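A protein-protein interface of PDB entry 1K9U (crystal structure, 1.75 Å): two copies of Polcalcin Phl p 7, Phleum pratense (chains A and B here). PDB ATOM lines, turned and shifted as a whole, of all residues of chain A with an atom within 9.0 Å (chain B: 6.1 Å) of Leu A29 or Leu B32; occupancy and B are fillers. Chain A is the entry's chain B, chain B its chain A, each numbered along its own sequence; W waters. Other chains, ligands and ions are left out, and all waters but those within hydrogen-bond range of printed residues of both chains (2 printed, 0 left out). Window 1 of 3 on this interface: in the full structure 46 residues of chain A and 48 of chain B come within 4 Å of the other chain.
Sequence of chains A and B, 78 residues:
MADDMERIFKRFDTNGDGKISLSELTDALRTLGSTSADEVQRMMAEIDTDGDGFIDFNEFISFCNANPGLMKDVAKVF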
ATOM      1  N   ARG A  11     -15.009  15.722 -27.598  1.00  0.00           N
ATOM      2  CA  ARG A  11     -14.861  16.944 -28.389  1.00  0.00           C
ATOM      3  C   ARG A  11     -14.003  17.952 -27.612  1.00  0.00           C
ATOM      4  O   ARG A  11     -13.232  18.708 -28.205  1.00  0.00           O
ATOM      5  CB  ARG A  11     -16.229  17.560 -28.704  1.00  0.00           C
ATOM      6  CG  ARG A  11     -17.057  16.796 -29.732  1.00  0.00           C
ATOM      7  CD  ARG A  11     -16.430  16.859 -31.122  1.00  0.00           C
ATOM      8  NE  ARG A  11     -16.382  18.221 -31.651  1.00  0.00           N
ATOM      9  CZ  ARG A  11     -17.448  18.915 -32.041  1.00  0.00           C
ATOM     10  NH1 ARG A  11     -18.660  18.380 -31.970  1.00  0.00           N
ATOM     11  NH2 ARG A  11     -17.305  20.151 -32.501  1.00  0.00           N
ATOM     12  N   PHE A  12     -14.142  17.953 -26.288  1.00  0.00           N
ATOM     13  CA  PHE A  12     -13.373  18.853 -25.424  1.00  0.00           C
ATOM     14  C   PHE A  12     -11.936  18.370 -25.246  1.00  0.00           C
ATOM     15  O   PHE A  12     -10.992  19.162 -25.275  1.00  0.00           O
ATOM     16  CB  PHE A  12     -14.001  18.953 -24.031  1.00  0.00           C
ATOM     17  CG  PHE A  12     -15.146  19.921 -23.932  1.00  0.00           C
ATOM     18  CD1 PHE A  12     -16.344  19.686 -24.597  1.00  0.00           C
ATOM     19  CD2 PHE A  12     -15.037  21.055 -23.131  1.00  0.00           C
ATOM     20  CE1 PHE A  12     -17.418  20.566 -24.466  1.00  0.00           C
ATOM     21  CE2 PHE A  12     -16.106  21.941 -22.992  1.00  0.00           C
ATOM     22  CZ  PHE A  12     -17.297  21.692 -23.660  1.00  0.00           C
ATOM     23  N   ILE A  20      -9.483  17.179 -19.436  1.00  0.00           N
ATOM     24  CA  ILE A  20      -9.673  18.441 -20.127  1.00  0.00           C
ATOM     25  C   ILE A  20      -8.796  19.484 -19.444  1.00  0.00           C
ATOM     26  O   ILE A  20      -8.967  19.779 -18.257  1.00  0.00           O
ATOM     27  CB  ILE A  20     -11.140  18.894 -20.075  1.00  0.00           C
ATOM     28  CG1 ILE A  20     -12.030  17.847 -20.758  1.00  0.00           C
ATOM     29  CG2 ILE A  20     -11.285  20.249 -20.758  1.00  0.00           C
ATOM     30  CD1 ILE A  20     -13.523  18.124 -20.642  1.00  0.00           C
ATOM     31  N   SER A  21      -7.856  20.028 -20.207  1.00  0.00           N
ATOM     32  CA  SER A  21      -6.924  21.022 -19.703  1.00  0.00           C
ATOM     33  C   SER A  21      -7.483  22.430 -19.837  1.00  0.00           C
ATOM     34  O   SER A  21      -8.567  22.634 -20.390  1.00  0.00           O
ATOM     35  CB  SER A  21      -5.612  20.934 -20.473  1.00  0.00           C
ATOM     36  OG  SER A  21      -5.818  21.301 -21.822  1.00  0.00           O
ATOM     37  N   LEU A  22      -6.724  23.400 -19.338  1.00  0.00           N
ATOM     38  CA  LEU A  22      -7.130  24.798 -19.397  1.00  0.00           C
ATOM     39  C   LEU A  22      -7.204  25.261 -20.844  1.00  0.00           C
ATOM     40  O   LEU A  22      -8.160  25.929 -21.248  1.00  0.00           O
ATOM     41  CB  LEU A  22      -6.138  25.673 -18.621  1.00  0.00           C
ATOM     42  CG  LEU A  22      -6.458  27.168 -18.663  1.00  0.00           C
ATOM     43  CD1 LEU A  22      -7.839  27.419 -18.070  1.00  0.00           C
ATOM     44  CD2 LEU A  22      -5.384  27.933 -17.900  1.00  0.00           C
ATOM     45  N   SER A  23      -6.186  24.910 -21.626  1.00  0.00           N
ATOM     46  CA  SER A  23      -6.157  25.293 -23.032  1.00  0.00           C
ATOM     47  C   SER A  23      -7.293  24.615 -23.797  1.00  0.00           C
ATOM     48  O   SER A  23      -7.894  25.214 -24.686  1.00  0.00           O
ATOM     49  CB  SER A  23      -4.796  24.947 -23.657  1.00  0.00           C
ATOM     50  OG  SER A  23      -4.457  23.580 -23.485  1.00  0.00           O
ATOM     51  N   GLU A  24      -7.592  23.366 -23.448  1.00  0.00           N
ATOM     52  CA  GLU A  24      -8.677  22.639 -24.105  1.00  0.00           C
ATOM     53  C   GLU A  24     -10.036  23.229 -23.747  1.00  0.00           C
ATOM     54  O   GLU A  24     -10.903  23.357 -24.612  1.00  0.00           O
ATOM     55  CB  GLU A  24      -8.640  21.152 -23.738  1.00  0.00           C
ATOM     56  CG  GLU A  24      -7.412  20.425 -24.290  1.00  0.00           C
ATOM     57  CD  GLU A  24      -7.348  18.977 -23.862  1.00  0.00           C
ATOM     58  OE1 GLU A  24      -7.768  18.672 -22.730  1.00  0.00           O
ATOM     59  OE2 GLU A  24      -6.861  18.141 -24.651  1.00  0.00           O
ATOM     60  N   LEU A  25     -10.228  23.601 -22.483  1.00  0.00           N
ATOM     61  CA  LEU A  25     -11.500  24.183 -22.065  1.00  0.00           C
ATOM     62  C   LEU A  25     -11.692  25.536 -22.739  1.00  0.00           C
ATOM     63  O   LEU A  25     -12.764  25.833 -23.266  1.00  0.00           O
ATOM     64  CB  LEU A  25     -11.554  24.354 -20.541  1.00  0.00           C
ATOM     65  CG  LEU A  25     -12.789  25.090 -19.990  1.00  0.00           C
ATOM     66  CD1 LEU A  25     -14.067  24.345 -20.379  1.00  0.00           C
ATOM     67  CD2 LEU A  25     -12.680  25.201 -18.471  1.00  0.00           C
ATOM     68  N   THR A  26     -10.643  26.350 -22.721  1.00  0.00           N
ATOM     69  CA  THR A  26     -10.685  27.669 -23.330  1.00  0.00           C
ATOM     70  C   THR A  26     -11.009  27.552 -24.815  1.00  0.00           C
ATOM     71  O   THR A  26     -11.851  28.288 -25.336  1.00  0.00           O
ATOM     72  CB  THR A  26      -9.334  28.394 -23.166  1.00  0.00           C
ATOM     73  OG1 THR A  26      -8.998  28.466 -21.775  1.00  0.00           O
ATOM     74  CG2 THR A  26      -9.412  29.803 -23.731  1.00  0.00           C
ATOM     75  N   ASP A  27     -10.341  26.624 -25.496  1.00  0.00           N
ATOM     76  CA  ASP A  27     -10.576  26.429 -26.920  1.00  0.00           C
ATOM     77  C   ASP A  27     -12.001  25.968 -27.200  1.00  0.00           C
ATOM     78  O   ASP A  27     -12.589  26.355 -28.208  1.00  0.00           O
ATOM     79  CB  ASP A  27      -9.568  25.429 -27.500  1.00  0.00           C
ATOM     80  CG  ASP A  27      -8.140  25.938 -27.421  1.00  0.00           C
ATOM     81  OD1 ASP A  27      -7.964  27.166 -27.288  1.00  0.00           O
ATOM     82  OD2 ASP A  27      -7.194  25.120 -27.498  1.00  0.00           O
ATOM     83  N   ALA A  28     -12.561  25.153 -26.308  1.00  0.00           N
ATOM     84  CA  ALA A  28     -13.927  24.677 -26.493  1.00  0.00           C
ATOM     85  C   ALA A  28     -14.909  25.836 -26.317  1.00  0.00           C
ATOM     86  O   ALA A  28     -15.893  25.937 -27.046  1.00  0.00           O
ATOM     87  CB  ALA A  28     -14.242  23.554 -25.502  1.00  0.00           C
ATOM     88  N   LEU A  29     -14.639  26.710 -25.351  1.00  0.00           N
ATOM     89  CA  LEU A  29     -15.500  27.864 -25.114  1.00  0.00           C
ATOM     90  C   LEU A  29     -15.471  28.800 -26.316  1.00  0.00           C
ATOM     91  O   LEU A  29     -16.485  29.405 -26.667  1.00  0.00           O
ATOM     92  CB  LEU A  29     -15.050  28.622 -23.860  1.00  0.00           C
ATOM     93  CG  LEU A  29     -15.343  27.922 -22.534  1.00  0.00           C
ATOM     94  CD1 LEU A  29     -14.692  28.688 -21.394  1.00  0.00           C
ATOM     95  CD2 LEU A  29     -16.854  27.825 -22.332  1.00  0.00           C
ATOM     96  N   ARG A  30     -14.302  28.911 -26.942  1.00  0.00           N
ATOM     97  CA  ARG A  30     -14.129  29.755 -28.121  1.00  0.00           C
ATOM     98  C   ARG A  30     -15.110  29.317 -29.210  1.00  0.00           C
ATOM     99  O   ARG A  30     -15.639  30.144 -29.953  1.00  0.00           O
ATOM    100  CB  ARG A  30     -12.696  29.636 -28.649  1.00  0.00           C
ATOM    101  CG  ARG A  30     -11.628  30.215 -27.734  1.00  0.00           C
ATOM    102  CD  ARG A  30     -11.424  31.699 -27.982  1.00  0.00           C
ATOM    103  NE  ARG A  30     -10.431  32.275 -27.078  1.00  0.00           N
ATOM    104  CZ  ARG A  30     -10.645  32.517 -25.789  1.00  0.00           C
ATOM    105  NH1 ARG A  30     -11.822  32.237 -25.245  1.00  0.00           N
ATOM    106  NH2 ARG A  30      -9.681  33.038 -25.040  1.00  0.00           N
ATOM    107  N   THR A  31     -15.346  28.012 -29.298  1.00  0.00           N
ATOM    108  CA  THR A  31     -16.263  27.464 -30.297  1.00  0.00           C
ATOM    109  C   THR A  31     -17.705  27.825 -29.959  1.00  0.00           C
ATOM    110  O   THR A  31     -18.491  28.187 -30.838  1.00  0.00           O
ATOM    111  CB  THR A  31     -16.145  25.929 -30.378  1.00  0.00           C
ATOM    112  OG1 THR A  31     -14.820  25.570 -30.794  1.00  0.00           O
ATOM    113  CG2 THR A  31     -17.162  25.367 -31.368  1.00  0.00           C
ATOM    114  N   LEU A  32     -18.043  27.726 -28.677  1.00  0.00           N
ATOM    115  CA  LEU A  32     -19.383  28.040 -28.201  1.00  0.00           C
ATOM    116  C   LEU A  32     -19.753  29.490 -28.479  1.00  0.00           C
ATOM    117  O   LEU A  32     -20.930  29.823 -28.618  1.00  0.00           O
ATOM    118  CB  LEU A  32     -19.482  27.766 -26.697  1.00  0.00           C
ATOM    119  CG  LEU A  32     -19.577  26.292 -26.298  1.00  0.00           C
ATOM    120  CD1 LEU A  32     -19.310  26.130 -24.810  1.00  0.00           C
ATOM    121  CD2 LEU A  32     -20.957  25.764 -26.661  1.00  0.00           C
ATOM    122  N   GLY A  33     -18.745  30.348 -28.562  1.00  0.00           N
ATOM    123  CA  GLY A  33     -18.998  31.753 -28.819  1.00  0.00           C
ATOM    124  C   GLY A  33     -19.029  32.111 -30.293  1.00  0.00           C
ATOM    125  O   GLY A  33     -19.209  33.276 -30.646  1.00  0.00           O
ATOM    126  N   SER A  34     -18.852  31.113 -31.154  1.00  0.00           N
ATOM    127  CA  SER A  34     -18.854  31.326 -32.602  1.00  0.00           C
ATOM    128  C   SER A  34     -20.046  30.603 -33.227  1.00  0.00           C
ATOM    129  O   SER A  34     -20.001  30.182 -34.383  1.00  0.00           O
ATOM    130  CB  SER A  34     -17.563  30.783 -33.211  1.00  0.00           C
ATOM    131  OG  SER A  34     -16.428  31.270 -32.519  1.00  0.00           O
ATOM    132  N   THR A  35     -21.110  30.468 -32.450  1.00  0.00           N
ATOM    133  CA  THR A  35     -22.310  29.778 -32.900  1.00  0.00           C
ATOM    134  C   THR A  35     -23.098  30.515 -33.974  1.00  0.00           C
ATOM    135  O   THR A  35     -23.074  31.744 -34.055  1.00  0.00           O
ATOM    136  CB  THR A  35     -23.248  29.502 -31.719  1.00  0.00           C
ATOM    137  OG1 THR A  35     -23.456  30.716 -30.989  1.00  0.00           O
ATOM    138  CG2 THR A  35     -22.641  28.449 -30.799  1.00  0.00           C
ATOM    139  N   MET A  43     -30.916  27.373 -28.626  1.00  0.00           N
ATOM    140  CA  MET A  43     -30.655  27.589 -27.209  1.00  0.00           C
ATOM    141  C   MET A  43     -31.792  28.418 -26.613  1.00  0.00           C
ATOM    142  O   MET A  43     -32.241  28.165 -25.492  1.00  0.00           O
ATOM    143  CB  MET A  43     -29.315  28.299 -27.010  1.00  0.00           C
ATOM    144  CG  MET A  43     -28.117  27.409 -27.298  1.00  0.00           C
ATOM    145  SD  MET A  43     -26.553  28.208 -26.920  1.00  0.00           S
ATOM    146  CE  MET A  43     -25.538  27.606 -28.251  1.00  0.00           C
ATOM    147  N   LEU A  70     -24.543  26.888 -13.781  1.00  0.00           N
ATOM    148  CA  LEU A  70     -24.507  28.117 -14.559  1.00  0.00           C
ATOM    149  C   LEU A  70     -23.967  29.269 -13.723  1.00  0.00           C
ATOM    150  O   LEU A  70     -23.076  29.997 -14.159  1.00  0.00           O
ATOM    151  CB  LEU A  70     -25.901  28.473 -15.086  1.00  0.00           C
ATOM    152  CG  LEU A  70     -25.958  29.736 -15.952  1.00  0.00           C
ATOM    153  CD1 LEU A  70     -24.995  29.599 -17.125  1.00  0.00           C
ATOM    154  CD2 LEU A  70     -27.383  29.951 -16.455  1.00  0.00           C
ATOM    155  N   ASP A  73     -20.426  27.775 -11.649  1.00  0.00           N
ATOM    156  CA  ASP A  73     -19.253  27.494 -12.465  1.00  0.00           C
ATOM    157  C   ASP A  73     -19.064  28.411 -13.670  1.00  0.00           C
ATOM    158  O   ASP A  73     -18.084  29.154 -13.751  1.00  0.00           O
ATOM    159  CB  ASP A  73     -19.297  26.039 -12.945  1.00  0.00           C
ATOM    160  CG  ASP A  73     -19.511  25.050 -11.808  1.00  0.00           C
ATOM    161  OD1 ASP A  73     -19.284  25.415 -10.634  1.00  0.00           O
ATOM    162  OD2 ASP A  73     -19.903  23.899 -12.093  1.00  0.00           O
ATOM    163  N   VAL A  74     -20.005  28.357 -14.607  1.00  0.00           N
ATOM    164  CA  VAL A  74     -19.919  29.158 -15.824  1.00  0.00           C
ATOM    165  C   VAL A  74     -19.853  30.667 -15.615  1.00  0.00           C
ATOM    166  O   VAL A  74     -19.041  31.345 -16.245  1.00  0.00           O
ATOM    167  CB  VAL A  74     -21.101  28.843 -16.772  1.00  0.00           C
ATOM    168  CG1 VAL A  74     -20.970  29.653 -18.058  1.00  0.00           C
ATOM    169  CG2 VAL A  74     -21.124  27.356 -17.084  1.00  0.00           C
ATOM    170  N   ALA A  75     -20.700  31.192 -14.736  1.00  0.00           N
ATOM    171  CA  ALA A  75     -20.735  32.627 -14.471  1.00  0.00           C
ATOM    172  C   ALA A  75     -19.415  33.164 -13.930  1.00  0.00           C
ATOM    173  O   ALA A  75     -19.097  34.338 -14.124  1.00  0.00           O
ATOM    174  CB  ALA A  75     -21.860  32.951 -13.497  1.00  0.00           C
ATOM    175  N   VAL A  77     -16.854  32.994 -15.029  1.00  0.00           N
ATOM    176  CA  VAL A  77     -16.108  33.440 -16.196  1.00  0.00           C
ATOM    177  C   VAL A  77     -16.276  34.943 -16.400  1.00  0.00           C
ATOM    178  O   VAL A  77     -15.294  35.668 -16.560  1.00  0.00           O
ATOM    179  CB  VAL A  77     -16.585  32.695 -17.464  1.00  0.00           C
ATOM    180  CG1 VAL A  77     -16.322  33.535 -18.699  1.00  0.00           C
ATOM    181  CG2 VAL A  77     -15.865  31.359 -17.578  1.00  0.00           C
ATOM    182  N   PHE A  78     -17.524  35.405 -16.393  1.00  0.00           N
ATOM    183  CA  PHE A  78     -17.807  36.823 -16.581  1.00  0.00           C
ATOM    184  C   PHE A  78     -17.265  37.648 -15.419  1.00  0.00           C
ATOM    185  O   PHE A  78     -16.711  37.048 -14.474  1.00  0.00           O
ATOM    186  CB  PHE A  78     -19.315  37.057 -16.716  1.00  0.00           C
ATOM    187  CG  PHE A  78     -19.980  36.177 -17.737  1.00  0.00           C
ATOM    188  CD1 PHE A  78     -19.395  35.964 -18.981  1.00  0.00           C
ATOM    189  CD2 PHE A  78     -21.204  35.575 -17.460  1.00  0.00           C
ATOM    190  CE1 PHE A  78     -20.020  35.163 -19.937  1.00  0.00           C
ATOM    191  CE2 PHE A  78     -21.836  34.773 -18.408  1.00  0.00           C
ATOM    192  CZ  PHE A  78     -21.244  34.566 -19.649  1.00  0.00           C
ATOM    193  OXT PHE A  78     -17.405  38.889 -15.466  1.00  0.00           O
ATOM    194  N   PHE B  12     -26.370  41.346 -19.634  1.00  0.00           N
ATOM    195  CA  PHE B  12     -26.698  40.995 -21.001  1.00  0.00           C
ATOM    196  C   PHE B  12     -28.018  41.523 -21.535  1.00  0.00           C
ATOM    197  O   PHE B  12     -28.294  41.406 -22.727  1.00  0.00           O
ATOM    198  CB  PHE B  12     -26.558  39.489 -21.175  1.00  0.00           C
ATOM    199  CG  PHE B  12     -25.134  39.024 -21.040  1.00  0.00           C
ATOM    200  CD1 PHE B  12     -24.156  39.498 -21.915  1.00  0.00           C
ATOM    201  CD2 PHE B  12     -24.752  38.175 -20.009  1.00  0.00           C
ATOM    202  CE1 PHE B  12     -22.816  39.135 -21.761  1.00  0.00           C
ATOM    203  CE2 PHE B  12     -23.417  37.806 -19.845  1.00  0.00           C
ATOM    204  CZ  PHE B  12     -22.447  38.289 -20.724  1.00  0.00           C
ATOM    205  N   ASP B  27     -24.894  37.932 -28.098  1.00  0.00           N
ATOM    206  CA  ASP B  27     -23.772  38.677 -27.537  1.00  0.00           C
ATOM    207  C   ASP B  27     -23.232  38.010 -26.271  1.00  0.00           C
ATOM    208  O   ASP B  27     -22.023  37.987 -26.051  1.00  0.00           O
ATOM    209  CB  ASP B  27     -24.178  40.119 -27.221  1.00  0.00           C
ATOM    210  CG  ASP B  27     -24.395  40.945 -28.466  1.00  0.00           C
ATOM    211  OD1 ASP B  27     -23.626  40.770 -29.436  1.00  0.00           O
ATOM    212  OD2 ASP B  27     -25.322  41.779 -28.469  1.00  0.00           O
ATOM    213  N   ALA B  28     -24.123  37.472 -25.443  1.00  0.00           N
ATOM    214  CA  ALA B  28     -23.693  36.800 -24.213  1.00  0.00           C
ATOM    215  C   ALA B  28     -22.827  35.596 -24.571  1.00  0.00           C
ATOM    216  O   ALA B  28     -21.804  35.339 -23.934  1.00  0.00           O
ATOM    217  CB  ALA B  28     -24.906  36.349 -23.391  1.00  0.00           C
ATOM    218  N   LEU B  29     -23.236  34.860 -25.597  1.00  0.00           N
ATOM    219  CA  LEU B  29     -22.468  33.699 -26.034  1.00  0.00           C
ATOM    220  C   LEU B  29     -21.109  34.113 -26.604  1.00  0.00           C
ATOM    221  O   LEU B  29     -20.097  33.457 -26.354  1.00  0.00           O
ATOM    222  CB  LEU B  29     -23.261  32.906 -27.072  1.00  0.00           C
ATOM    223  CG  LEU B  29     -24.507  32.218 -26.509  1.00  0.00           C
ATOM    224  CD1 LEU B  29     -25.329  31.602 -27.629  1.00  0.00           C
ATOM    225  CD2 LEU B  29     -24.074  31.157 -25.510  1.00  0.00           C
ATOM    226  N   ARG B  30     -21.081  35.208 -27.356  1.00  0.00           N
ATOM    227  CA  ARG B  30     -19.829  35.673 -27.933  1.00  0.00           C
ATOM    228  C   ARG B  30     -18.890  36.192 -26.853  1.00  0.00           C
ATOM    229  O   ARG B  30     -17.671  36.175 -27.019  1.00  0.00           O
ATOM    230  CB  ARG B  30     -20.088  36.769 -28.966  1.00  0.00           C
ATOM    231  CG  ARG B  30     -21.011  36.338 -30.090  1.00  0.00           C
ATOM    232  CD  ARG B  30     -20.650  37.022 -31.400  1.00  0.00           C
ATOM    233  NE  ARG B  30     -21.563  36.662 -32.482  1.00  0.00           N
ATOM    234  CZ  ARG B  30     -21.837  35.416 -32.855  1.00  0.00           C
ATOM    235  NH1 ARG B  30     -21.273  34.388 -32.235  1.00  0.00           N
ATOM    236  NH2 ARG B  30     -22.677  35.196 -33.856  1.00  0.00           N
ATOM    237  N   THR B  31     -19.461  36.651 -25.743  1.00  0.00           N
ATOM    238  CA  THR B  31     -18.665  37.164 -24.631  1.00  0.00           C
ATOM    239  C   THR B  31     -18.000  35.973 -23.955  1.00  0.00           C
ATOM    240  O   THR B  31     -16.804  35.989 -23.661  1.00  0.00           O
ATOM    241  CB  THR B  31     -19.541  37.894 -23.596  1.00  0.00           C
ATOM    242  OG1 THR B  31     -20.054  39.099 -24.172  1.00  0.00           O
ATOM    243  CG2 THR B  31     -18.733  38.240 -22.353  1.00  0.00           C
ATOM    244  N   LEU B  32     -18.797  34.941 -23.712  1.00  0.00           N
ATOM    245  CA  LEU B  32     -18.305  33.718 -23.097  1.00  0.00           C
ATOM    246  C   LEU B  32     -17.181  33.167 -23.963  1.00  0.00           C
ATOM    247  O   LEU B  32     -16.156  32.706 -23.457  1.00  0.00           O
ATOM    248  CB  LEU B  32     -19.447  32.702 -22.989  1.00  0.00           C
ATOM    249  CG  LEU B  32     -19.136  31.238 -22.666  1.00  0.00           C
ATOM    250  CD1 LEU B  32     -20.377  30.571 -22.092  1.00  0.00           C
ATOM    251  CD2 LEU B  32     -18.674  30.515 -23.928  1.00  0.00           C
ATOM    252  N   GLY B  33     -17.378  33.245 -25.276  1.00  0.00           N
ATOM    253  CA  GLY B  33     -16.391  32.748 -26.216  1.00  0.00           C
ATOM    254  C   GLY B  33     -15.075  33.503 -26.254  1.00  0.00           C
ATOM    255  O   GLY B  33     -14.052  32.933 -26.630  1.00  0.00           O
ATOM    256  N   SER B  34     -15.086  34.780 -25.877  1.00  0.00           N
ATOM    257  CA  SER B  34     -13.862  35.579 -25.886  1.00  0.00           C
ATOM    258  C   SER B  34     -13.280  35.717 -24.481  1.00  0.00           C
ATOM    259  O   SER B  34     -12.556  36.668 -24.183  1.00  0.00           O
ATOM    260  CB  SER B  34     -14.138  36.968 -26.468  1.00  0.00           C
ATOM    261  OG  SER B  34     -15.082  37.675 -25.683  1.00  0.00           O
ATOM    262  N   THR B  35     -13.603  34.753 -23.628  1.00  0.00           N
ATOM    263  CA  THR B  35     -13.132  34.735 -22.249  1.00  0.00           C
ATOM    264  C   THR B  35     -11.647  34.401 -22.152  1.00  0.00           C
ATOM    265  O   THR B  35     -11.168  33.473 -22.804  1.00  0.00           O
ATOM    266  CB  THR B  35     -13.915  33.698 -21.422  1.00  0.00           C
ATOM    267  OG1 THR B  35     -15.299  34.069 -21.379  1.00  0.00           O
ATOM    268  CG2 THR B  35     -13.369  33.618 -20.010  1.00  0.00           C
ATOM    269  N   VAL B  40     -11.324  31.741 -17.425  1.00  0.00           N
ATOM    270  CA  VAL B  40     -11.676  30.347 -17.655  1.00  0.00           C
ATOM    271  C   VAL B  40     -11.153  29.495 -16.508  1.00  0.00           C
ATOM    272  O   VAL B  40     -11.768  28.496 -16.130  1.00  0.00           O
ATOM    273  CB  VAL B  40     -11.089  29.831 -18.992  1.00  0.00           C
ATOM    274  CG1 VAL B  40     -11.406  28.361 -19.169  1.00  0.00           C
ATOM    275  CG2 VAL B  40     -11.665  30.635 -20.152  1.00  0.00           C
ATOM    276  N   MET B  43     -13.588  29.041 -13.716  1.00  0.00           N
ATOM    277  CA  MET B  43     -14.655  28.108 -14.054  1.00  0.00           C
ATOM    278  C   MET B  43     -14.080  26.702 -13.901  1.00  0.00           C
ATOM    279  O   MET B  43     -14.715  25.807 -13.340  1.00  0.00           O
ATOM    280  CB  MET B  43     -15.112  28.320 -15.499  1.00  0.00           C
ATOM    281  CG  MET B  43     -16.232  27.392 -15.913  1.00  0.00           C
ATOM    282  SD  MET B  43     -16.621  27.511 -17.669  1.00  0.00           S
ATOM    283  CE  MET B  43     -17.175  25.834 -17.980  1.00  0.00           C
ATOM    284  N   PHE B  78     -21.705  21.105 -29.741  1.00  0.00           N
ATOM    285  CA  PHE B  78     -20.881  19.900 -29.741  1.00  0.00           C
ATOM    286  C   PHE B  78     -21.752  18.657 -29.878  1.00  0.00           C
ATOM    287  O   PHE B  78     -21.577  17.721 -29.070  1.00  0.00           O
ATOM    288  CB  PHE B  78     -20.060  19.807 -28.450  1.00  0.00           C
ATOM    289  CG  PHE B  78     -19.144  20.974 -28.225  1.00  0.00           C
ATOM    290  CD1 PHE B  78     -19.645  22.197 -27.790  1.00  0.00           C
ATOM    291  CD2 PHE B  78     -17.778  20.857 -28.460  1.00  0.00           C
ATOM    292  CE1 PHE B  78     -18.800  23.285 -27.592  1.00  0.00           C
ATOM    293  CE2 PHE B  78     -16.923  21.941 -28.266  1.00  0.00           C
ATOM    294  CZ  PHE B  78     -17.437  23.158 -27.830  1.00  0.00           C
ATOM    295  OXT PHE B  78     -22.594  18.628 -30.799  1.00  0.00           O
HETATM  296  O   HOH W   1     -24.961  34.017 -34.313  1.00  0.00           O
HETATM  297  O   HOH W   2     -20.592  33.418 -35.245  1.00  0.00           O
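O of Gly A33 sits at hydrogen-bond distance from NH1 of Arg B30 (2.8 Å).
NH2 of Arg B30 lies within hydrogen-bond range of O of Thr A35.
O of Gly B33 is in hydrogen-bond range of NH1 of Arg A30 (2.7 Å).
The backbone carbonyl oxygen (O) of Thr B35 lies within hydrogen-bond range of the guanidinium group (NH2) of Arg A30, at 2.7 Å.
The backbone carbonyl oxygen (O) of Arg B30 is in hydrogen-bond range of the side-chain hydroxyl (OG) of Ser B34.
The backbone carbonyl oxygen (O) of Thr B31 lies within hydrogen-bond range of the side-chain hydroxyl (OG) of Ser B34, at 3.1 Å.
The backbone carbonyl oxygen of Thr B31 is in hydrogen-bond range of the side-chain hydroxyl of Thr B35.
O of Leu B32 lies within hydrogen-bond range of OG1 of Thr B35, 2.6 Å away.
The backbone carbonyl oxygen (O) of Leu A22 sits at hydrogen-bond distance from the side-chain hydroxyl (OG1) of Thr A26, 2.7 Å away.
The backbone carbonyl oxygen (O) of Arg A30 lies within hydrogen-bond range of the side-chain hydroxyl (OG) of Ser A34 (2.9 Å).
Among the printed residues, merely in contact across the chains: Val A77 with Thr B35 (2.9 Å), Gly A33 with Leu B29 (3.2 Å), Ala A28 with Phe B78 (3.3 Å), Asp A73 with Met B43 (3.3 Å), Leu A32 with Phe B78 (3.4 Å), Leu A29 with Gly B33 (3.4 Å), Leu A25 with Val B40 (3.5 Å), Arg A11 with Phe B78 (3.5 Å), Thr A26 with Val B40 (3.5 Å), Leu A29 with Leu B32 (3.6 Å), Met A43 with Leu B29 (3.7 Å), Phe A78 with Phe B12 (3.7 Å), Val A77 with Met B43 (3.8 Å), Leu A29 with Val B40 (3.8 Å), Gly A33 with Gly B33 (3.8 Å), Leu A22 with Val B40 (3.8 Å), Arg A30 with Ser B34 (3.8 Å), Phe A78 with Leu B32 (3.9 Å), Ser A34 with Arg B30 (3.9 Å), Thr A35 with Leu B29 (3.9 Å), Thr A31 with Phe B78 (3.98 Å) and Leu A32 with Leu B32 (3.98 Å).
Printed residues of chain B within 4 Å of Leu A25: Val B40.
Of the printed residues of chain B, Gly A33 touches Leu B29, Arg B30 and Gly B33.
Of the printed residues of chain B, Met A43 touches Leu B29 (3.7 Å).
Printed residues of chain A within 4 Å of Phe B12: Phe A78.
No residue of chain A comes within 4 Å of Thr B31.
Of the printed residues of chain A, Leu B32 touches Leu A29 (3.6 Å), Leu A32 (3.98 Å) and Phe A78 (3.9 Å).
Of the printed residues of chain A, Ser B34 touches Arg A30.
The nearest residue of chain B that does not touch Leu A29 is Met B43 (4.4 Å).
Printed residues of chain B that touch a printed residue of chain A: Phe B12, Leu B29, Arg B30, Leu B32, Gly B33, Ser B34, Thr B35, Val B40, Met B43 and Phe B78.
Ala A28 touches Phe B78, but with the chains exchanged Phe A78 does not touch Ala B28 (4.4 Å).
Leu A29 touches Leu B32, but with the chains exchanged Leu A32 does not touch Leu B29 (4.2 Å).
Arg A30 touches Gly B33, and with the chains exchanged Gly A33 touches Arg B30.
Gly A33 touches its own counterpart, Gly B33.
Of the 26 pairs that touch across the chains among the printed residues, 12 have their exchanged pair printed and touching as well.
Water W1 bridges NH2 of Arg B30 and O of Thr A35.
Water W2 lies within hydrogen-bond range of NH2 of Arg B30 (3.1 Å), O of Thr A35 (3.2 Å) and O of Ser A34 (3.4 Å).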
